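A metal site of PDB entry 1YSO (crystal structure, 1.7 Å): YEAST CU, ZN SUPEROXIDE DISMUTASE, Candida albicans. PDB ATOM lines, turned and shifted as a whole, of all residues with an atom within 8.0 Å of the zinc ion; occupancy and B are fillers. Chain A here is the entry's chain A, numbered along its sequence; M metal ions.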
ATOM      1  N   PHE A  45     -21.348  31.551 -13.992  1.00  0.00           N
ATOM      2  CA  PHE A  45     -22.383  32.078 -13.124  1.00  0.00           C
ATOM      3  C   PHE A  45     -23.727  31.537 -13.597  1.00  0.00           C
ATOM      4  O   PHE A  45     -24.156  31.873 -14.725  1.00  0.00           O
ATOM      5  CB  PHE A  45     -22.282  33.577 -13.251  1.00  0.00           C
ATOM      6  CG  PHE A  45     -23.119  34.441 -12.335  1.00  0.00           C
ATOM      7  CD1 PHE A  45     -23.238  34.165 -10.971  1.00  0.00           C
ATOM      8  CD2 PHE A  45     -23.782  35.529 -12.875  1.00  0.00           C
ATOM      9  CE1 PHE A  45     -23.978  35.010 -10.133  1.00  0.00           C
ATOM     10  CE2 PHE A  45     -24.514  36.369 -12.033  1.00  0.00           C
ATOM     11  CZ  PHE A  45     -24.630  36.107 -10.679  1.00  0.00           C
ATOM     12  N   HIS A  46     -24.425  30.693 -12.850  1.00  0.00           N
ATOM     13  CA  HIS A  46     -25.665  30.115 -13.347  1.00  0.00           C
ATOM     14  C   HIS A  46     -26.708  29.934 -12.271  1.00  0.00           C
ATOM     15  O   HIS A  46     -26.401  29.924 -11.076  1.00  0.00           O
ATOM     16  CB  HIS A  46     -25.467  28.715 -13.929  1.00  0.00           C
ATOM     17  CG  HIS A  46     -24.134  28.462 -14.632  1.00  0.00           C
ATOM     18  ND1 HIS A  46     -23.199  27.640 -14.183  1.00  0.00           N
ATOM     19  CD2 HIS A  46     -23.710  29.047 -15.805  1.00  0.00           C
ATOM     20  CE1 HIS A  46     -22.213  27.711 -15.050  1.00  0.00           C
ATOM     21  NE2 HIS A  46     -22.535  28.550 -16.009  1.00  0.00           N
ATOM     22  N   ILE A  47     -27.958  29.743 -12.716  1.00  0.00           N
ATOM     23  CA  ILE A  47     -29.015  29.338 -11.814  1.00  0.00           C
ATOM     24  C   ILE A  47     -29.151  27.836 -11.985  1.00  0.00           C
ATOM     25  O   ILE A  47     -29.209  27.307 -13.101  1.00  0.00           O
ATOM     26  CB  ILE A  47     -30.322  30.038 -12.163  1.00  0.00           C
ATOM     27  CG1 ILE A  47     -30.060  31.537 -11.971  1.00  0.00           C
ATOM     28  CG2 ILE A  47     -31.480  29.525 -11.308  1.00  0.00           C
ATOM     29  CD1 ILE A  47     -31.170  32.533 -12.294  1.00  0.00           C
ATOM     30  N   HIS A  48     -29.083  27.134 -10.865  1.00  0.00           N
ATOM     31  CA  HIS A  48     -29.181  25.697 -10.800  1.00  0.00           C
ATOM     32  C   HIS A  48     -30.593  25.355 -10.361  1.00  0.00           C
ATOM     33  O   HIS A  48     -31.302  26.182  -9.766  1.00  0.00           O
ATOM     34  CB  HIS A  48     -28.130  25.167  -9.827  1.00  0.00           C
ATOM     35  CG  HIS A  48     -26.759  25.068 -10.444  1.00  0.00           C
ATOM     36  ND1 HIS A  48     -26.000  24.009 -10.560  1.00  0.00           N
ATOM     37  CD2 HIS A  48     -26.072  26.111 -11.008  1.00  0.00           C
ATOM     38  CE1 HIS A  48     -24.885  24.356 -11.159  1.00  0.00           C
ATOM     39  NE2 HIS A  48     -24.930  25.626 -11.438  1.00  0.00           N
ATOM     40  N   PRO A  62     -28.304  20.322 -11.313  1.00  0.00           N
ATOM     41  CA  PRO A  62     -27.880  20.785 -12.633  1.00  0.00           C
ATOM     42  C   PRO A  62     -28.360  22.198 -12.931  1.00  0.00           C
ATOM     43  O   PRO A  62     -29.135  22.786 -12.148  1.00  0.00           O
ATOM     44  CB  PRO A  62     -28.479  19.750 -13.544  1.00  0.00           C
ATOM     45  CG  PRO A  62     -29.828  19.560 -12.894  1.00  0.00           C
ATOM     46  CD  PRO A  62     -29.412  19.374 -11.449  1.00  0.00           C
ATOM     47  N   HIS A  63     -27.950  22.771 -14.077  1.00  0.00           N
ATOM     48  CA  HIS A  63     -28.436  24.063 -14.514  1.00  0.00           C
ATOM     49  C   HIS A  63     -29.948  23.979 -14.719  1.00  0.00           C
ATOM     50  O   HIS A  63     -30.475  22.953 -15.177  1.00  0.00           O
ATOM     51  CB  HIS A  63     -27.825  24.495 -15.830  1.00  0.00           C
ATOM     52  CG  HIS A  63     -26.329  24.750 -15.790  1.00  0.00           C
ATOM     53  ND1 HIS A  63     -25.593  25.028 -16.834  1.00  0.00           N
ATOM     54  CD2 HIS A  63     -25.519  24.720 -14.684  1.00  0.00           C
ATOM     55  CE1 HIS A  63     -24.349  25.169 -16.413  1.00  0.00           C
ATOM     56  NE2 HIS A  63     -24.306  24.991 -15.117  1.00  0.00           N
ATOM     57  N   PHE A  64     -30.644  25.056 -14.371  1.00  0.00           N
ATOM     58  CA  PHE A  64     -32.089  25.091 -14.505  1.00  0.00           C
ATOM     59  C   PHE A  64     -32.357  25.110 -16.010  1.00  0.00           C
ATOM     60  O   PHE A  64     -31.925  26.001 -16.754  1.00  0.00           O
ATOM     61  CB  PHE A  64     -32.652  26.337 -13.806  1.00  0.00           C
ATOM     62  CG  PHE A  64     -34.183  26.412 -13.878  1.00  0.00           C
ATOM     63  CD1 PHE A  64     -34.988  25.298 -13.626  1.00  0.00           C
ATOM     64  CD2 PHE A  64     -34.786  27.639 -14.197  1.00  0.00           C
ATOM     65  CE1 PHE A  64     -36.383  25.392 -13.730  1.00  0.00           C
ATOM     66  CE2 PHE A  64     -36.184  27.720 -14.290  1.00  0.00           C
ATOM     67  CZ  PHE A  64     -36.970  26.600 -14.050  1.00  0.00           C
ATOM     68  N   ASN A  65     -33.082  24.085 -16.429  1.00  0.00           N
ATOM     69  CA  ASN A  65     -33.274  23.791 -17.840  1.00  0.00           C
ATOM     70  C   ASN A  65     -34.677  23.230 -18.087  1.00  0.00           C
ATOM     71  O   ASN A  65     -34.781  22.088 -18.559  1.00  0.00           O
ATOM     72  CB  ASN A  65     -32.178  22.789 -18.254  1.00  0.00           C
ATOM     73  CG  ASN A  65     -32.095  22.448 -19.721  1.00  0.00           C
ATOM     74  OD1 ASN A  65     -32.520  23.193 -20.611  1.00  0.00           O
ATOM     75  ND2 ASN A  65     -31.502  21.322 -20.074  1.00  0.00           N
ATOM     76  N   LYS A  69     -32.717  22.015 -23.259  1.00  0.00           N
ATOM     77  CA  LYS A  69     -31.777  22.444 -24.276  1.00  0.00           C
ATOM     78  C   LYS A  69     -30.342  22.241 -23.815  1.00  0.00           C
ATOM     79  O   LYS A  69     -30.121  21.739 -22.704  1.00  0.00           O
ATOM     80  CB  LYS A  69     -32.058  23.920 -24.591  1.00  0.00           C
ATOM     81  CG  LYS A  69     -33.415  23.999 -25.293  1.00  0.00           C
ATOM     82  CD  LYS A  69     -33.585  25.233 -26.119  1.00  0.00           C
ATOM     83  CE  LYS A  69     -34.916  25.144 -26.851  1.00  0.00           C
ATOM     84  NZ  LYS A  69     -35.119  26.408 -27.557  1.00  0.00           N
ATOM     85  N   THR A  70     -29.353  22.486 -24.644  1.00  0.00           N
ATOM     86  CA  THR A  70     -27.986  22.351 -24.220  1.00  0.00           C
ATOM     87  C   THR A  70     -27.480  23.676 -23.664  1.00  0.00           C
ATOM     88  O   THR A  70     -28.085  24.725 -23.841  1.00  0.00           O
ATOM     89  CB  THR A  70     -27.092  21.895 -25.400  1.00  0.00           C
ATOM     90  OG1 THR A  70     -27.363  22.720 -26.529  1.00  0.00           O
ATOM     91  CG2 THR A  70     -27.328  20.420 -25.686  1.00  0.00           C
ATOM     92  N   HIS A  71     -26.353  23.569 -22.968  1.00  0.00           N
ATOM     93  CA  HIS A  71     -25.677  24.708 -22.361  1.00  0.00           C
ATOM     94  C   HIS A  71     -25.211  25.711 -23.402  1.00  0.00           C
ATOM     95  O   HIS A  71     -24.724  25.307 -24.457  1.00  0.00           O
ATOM     96  CB  HIS A  71     -24.495  24.143 -21.551  1.00  0.00           C
ATOM     97  CG  HIS A  71     -23.821  25.224 -20.738  1.00  0.00           C
ATOM     98  ND1 HIS A  71     -24.267  25.814 -19.632  1.00  0.00           N
ATOM     99  CD2 HIS A  71     -22.660  25.815 -21.130  1.00  0.00           C
ATOM    100  CE1 HIS A  71     -23.388  26.748 -19.345  1.00  0.00           C
ATOM    101  NE2 HIS A  71     -22.465  26.734 -20.249  1.00  0.00           N
ATOM    102  N   GLY A  72     -25.294  27.014 -23.146  1.00  0.00           N
ATOM    103  CA  GLY A  72     -24.876  28.017 -24.098  1.00  0.00           C
ATOM    104  C   GLY A  72     -24.539  29.291 -23.375  1.00  0.00           C
ATOM    105  O   GLY A  72     -24.454  29.356 -22.151  1.00  0.00           O
ATOM    106  N   ALA A  73     -24.299  30.326 -24.183  1.00  0.00           N
ATOM    107  CA  ALA A  73     -24.040  31.647 -23.645  1.00  0.00           C
ATOM    108  C   ALA A  73     -25.382  32.334 -23.430  1.00  0.00           C
ATOM    109  O   ALA A  73     -26.350  31.964 -24.099  1.00  0.00           O
ATOM    110  CB  ALA A  73     -23.204  32.454 -24.646  1.00  0.00           C
ATOM    111  N   ARG A  79     -29.782  27.573 -25.112  1.00  0.00           N
ATOM    112  CA  ARG A  79     -29.153  27.807 -23.818  1.00  0.00           C
ATOM    113  C   ARG A  79     -30.121  27.313 -22.768  1.00  0.00           C
ATOM    114  O   ARG A  79     -31.299  27.072 -23.044  1.00  0.00           O
ATOM    115  CB  ARG A  79     -28.871  29.286 -23.635  1.00  0.00           C
ATOM    116  CG  ARG A  79     -29.996  30.252 -23.906  1.00  0.00           C
ATOM    117  CD  ARG A  79     -29.513  31.526 -23.291  1.00  0.00           C
ATOM    118  NE  ARG A  79     -29.893  31.513 -21.911  1.00  0.00           N
ATOM    119  CZ  ARG A  79     -30.279  32.580 -21.203  1.00  0.00           C
ATOM    120  NH1 ARG A  79     -30.365  33.854 -21.582  1.00  0.00           N
ATOM    121  NH2 ARG A  79     -30.625  32.321 -19.965  1.00  0.00           N
ATOM    122  N   HIS A  80     -29.546  26.945 -21.638  1.00  0.00           N
ATOM    123  CA  HIS A  80     -30.375  26.587 -20.505  1.00  0.00           C
ATOM    124  C   HIS A  80     -31.016  27.879 -19.991  1.00  0.00           C
ATOM    125  O   HIS A  80     -30.325  28.906 -20.050  1.00  0.00           O
ATOM    126  CB  HIS A  80     -29.567  25.995 -19.352  1.00  0.00           C
ATOM    127  CG  HIS A  80     -28.767  24.742 -19.645  1.00  0.00           C
ATOM    128  ND1 HIS A  80     -27.579  24.409 -19.170  1.00  0.00           N
ATOM    129  CD2 HIS A  80     -29.236  23.687 -20.398  1.00  0.00           C
ATOM    130  CE1 HIS A  80     -27.329  23.176 -19.572  1.00  0.00           C
ATOM    131  NE2 HIS A  80     -28.330  22.763 -20.319  1.00  0.00           N
ATOM    132  N   VAL A  81     -32.240  27.956 -19.445  1.00  0.00           N
ATOM    133  CA  VAL A  81     -32.737  29.177 -18.784  1.00  0.00           C
ATOM    134  C   VAL A  81     -31.730  29.752 -17.756  1.00  0.00           C
ATOM    135  O   VAL A  81     -31.566  30.959 -17.668  1.00  0.00           O
ATOM    136  CB  VAL A  81     -34.069  28.855 -18.031  1.00  0.00           C
ATOM    137  CG1 VAL A  81     -34.489  30.021 -17.113  1.00  0.00           C
ATOM    138  CG2 VAL A  81     -35.143  28.565 -19.074  1.00  0.00           C
ATOM    139  N   GLY A  82     -31.068  28.889 -16.980  1.00  0.00           N
ATOM    140  CA  GLY A  82     -30.153  29.329 -15.920  1.00  0.00           C
ATOM    141  C   GLY A  82     -28.781  29.832 -16.360  1.00  0.00           C
ATOM    142  O   GLY A  82     -27.963  30.213 -15.527  1.00  0.00           O
ATOM    143  N   ASP A  83     -28.456  29.824 -17.642  1.00  0.00           N
ATOM    144  CA  ASP A  83     -27.153  30.244 -18.110  1.00  0.00           C
ATOM    145  C   ASP A  83     -26.991  31.765 -18.139  1.00  0.00           C
ATOM    146  O   ASP A  83     -27.592  32.473 -18.937  1.00  0.00           O
ATOM    147  CB  ASP A  83     -26.920  29.664 -19.512  1.00  0.00           C
ATOM    148  CG  ASP A  83     -26.735  28.151 -19.544  1.00  0.00           C
ATOM    149  OD1 ASP A  83     -26.521  27.488 -18.510  1.00  0.00           O
ATOM    150  OD2 ASP A  83     -26.832  27.612 -20.636  1.00  0.00           O
ATOM    151  N   MET A  84     -26.158  32.234 -17.194  1.00  0.00           N
ATOM    152  CA  MET A  84     -25.844  33.652 -17.141  1.00  0.00           C
ATOM    153  C   MET A  84     -24.397  33.892 -17.575  1.00  0.00           C
ATOM    154  O   MET A  84     -23.892  34.969 -17.338  1.00  0.00           O
ATOM    155  CB  MET A  84     -26.079  34.187 -15.702  1.00  0.00           C
ATOM    156  CG  MET A  84     -27.505  33.953 -15.291  1.00  0.00           C
ATOM    157  SD  MET A  84     -27.929  34.660 -13.688  1.00  0.00           S
ATOM    158  CE  MET A  84     -26.975  33.613 -12.648  1.00  0.00           C
ATOM    159  N   GLY A  85     -23.690  32.961 -18.212  1.00  0.00           N
ATOM    160  CA  GLY A  85     -22.364  33.221 -18.738  1.00  0.00           C
ATOM    161  C   GLY A  85     -21.250  33.315 -17.693  1.00  0.00           C
ATOM    162  O   GLY A  85     -21.269  32.552 -16.734  1.00  0.00           O
ATOM    163  N   ASP A 124     -16.606  29.467 -17.768  1.00  0.00           N
ATOM    164  CA  ASP A 124     -17.601  28.713 -18.513  1.00  0.00           C
ATOM    165  C   ASP A 124     -17.190  28.826 -19.975  1.00  0.00           C
ATOM    166  O   ASP A 124     -17.086  29.923 -20.504  1.00  0.00           O
ATOM    167  CB  ASP A 124     -18.947  29.374 -18.239  1.00  0.00           C
ATOM    168  CG  ASP A 124     -20.185  28.782 -18.855  1.00  0.00           C
ATOM    169  OD1 ASP A 124     -20.057  28.012 -19.798  1.00  0.00           O
ATOM    170  OD2 ASP A 124     -21.267  29.118 -18.423  1.00  0.00           O
ATOM    171  N   GLY A 127     -20.461  26.456 -23.862  1.00  0.00           N
ATOM    172  CA  GLY A 127     -20.936  25.321 -24.649  1.00  0.00           C
ATOM    173  C   GLY A 127     -20.175  25.155 -25.948  1.00  0.00           C
ATOM    174  O   GLY A 127     -20.606  24.410 -26.839  1.00  0.00           O
ATOM    175  N   SER A 134     -19.095  20.196 -22.119  1.00  0.00           N
ATOM    176  CA  SER A 134     -19.275  21.577 -22.494  1.00  0.00           C
ATOM    177  C   SER A 134     -20.753  21.862 -22.749  1.00  0.00           C
ATOM    178  O   SER A 134     -21.241  22.928 -22.383  1.00  0.00           O
ATOM    179  CB  SER A 134     -18.433  21.790 -23.716  1.00  0.00           C
ATOM    180  OG  SER A 134     -18.631  23.054 -24.310  1.00  0.00           O
ATOM    181  N   LEU A 135     -21.488  20.868 -23.261  1.00  0.00           N
ATOM    182  CA  LEU A 135     -22.897  21.048 -23.560  1.00  0.00           C
ATOM    183  C   LEU A 135     -23.794  20.845 -22.350  1.00  0.00           C
ATOM    184  O   LEU A 135     -25.013  20.972 -22.449  1.00  0.00           O
ATOM    185  CB  LEU A 135     -23.308  20.080 -24.651  1.00  0.00           C
ATOM    186  CG  LEU A 135     -22.692  20.224 -26.028  1.00  0.00           C
ATOM    187  CD1 LEU A 135     -23.223  19.129 -26.938  1.00  0.00           C
ATOM    188  CD2 LEU A 135     -23.031  21.578 -26.590  1.00  0.00           C
ATOM    189  N   LYS A 136     -23.183  20.469 -21.220  1.00  0.00           N
ATOM    190  CA  LYS A 136     -23.919  20.291 -19.990  1.00  0.00           C
ATOM    191  C   LYS A 136     -23.609  21.371 -18.984  1.00  0.00           C
ATOM    192  O   LYS A 136     -24.549  21.951 -18.440  1.00  0.00           O
ATOM    193  CB  LYS A 136     -23.605  18.962 -19.304  1.00  0.00           C
ATOM    194  CG  LYS A 136     -24.242  17.770 -20.002  1.00  0.00           C
ATOM    195  CD  LYS A 136     -24.024  16.491 -19.189  1.00  0.00           C
ATOM    196  CE  LYS A 136     -24.588  15.309 -20.020  1.00  0.00           C
ATOM    197  NZ  LYS A 136     -24.336  14.008 -19.399  1.00  0.00           N
ATOM    198  N   THR A 137     -22.336  21.649 -18.685  1.00  0.00           N
ATOM    199  CA  THR A 137     -21.985  22.604 -17.644  1.00  0.00           C
ATOM    200  C   THR A 137     -21.130  23.757 -18.129  1.00  0.00           C
ATOM    201  O   THR A 137     -20.864  24.719 -17.407  1.00  0.00           O
ATOM    202  CB  THR A 137     -21.232  21.882 -16.506  1.00  0.00           C
ATOM    203  OG1 THR A 137     -19.972  21.452 -17.066  1.00  0.00           O
ATOM    204  CG2 THR A 137     -21.951  20.662 -15.999  1.00  0.00           C
ATOM    205  N   GLY A 138     -20.614  23.641 -19.351  1.00  0.00           N
ATOM    206  CA  GLY A 138     -19.661  24.628 -19.845  1.00  0.00           C
ATOM    207  C   GLY A 138     -18.302  24.378 -19.204  1.00  0.00           C
ATOM    208  O   GLY A 138     -17.446  25.241 -19.323  1.00  0.00           O
HETATM  209 ZN    ZN M   1     -26.086  25.651 -18.526  1.00  0.00          ZN
HETATM  210 CU    CU M   2     -23.288  26.325 -12.707  1.00  0.00          CU
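Of the 27 residues printed, 4 come within 4 Å of the zinc ion.
The nearest printed residue that does not touch the zinc ion is Lys 136 (4.01 Å).
The zinc ion is bound by ND1 of His 63, OD1 of Asp 83, ND1 of His 80 and ND1 of His 71.
The zinc ion has four donor atoms within binding distance.
ND1 of His 46 lies close to NE2 of His 63 (3.0 Å).
N of Gly 72 sits at hydrogen-bond distance from OD2 of Asp 83, at 3.0 Å.
O of Asp 83 lies within hydrogen-bond range of NH2 of Arg 79, 3.2 Å away.
The backbone NH (N) of His 80 sits at hydrogen-bond distance from the backbone carbonyl oxygen (O) of Thr 70.
NE2 of His 80 sits close to ND2 of Asn 65, 3.5 Å away.
NE2 of His 80 lies close to O of Lys 69 (3.2 Å).
NE2 of His 71 sits at hydrogen-bond distance from OD1 of Asp 124 (2.8 Å).
The backbone NH (N) of His 71 is in hydrogen-bond range of the backbone carbonyl oxygen (O) of Leu 135, 3.0 Å away.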
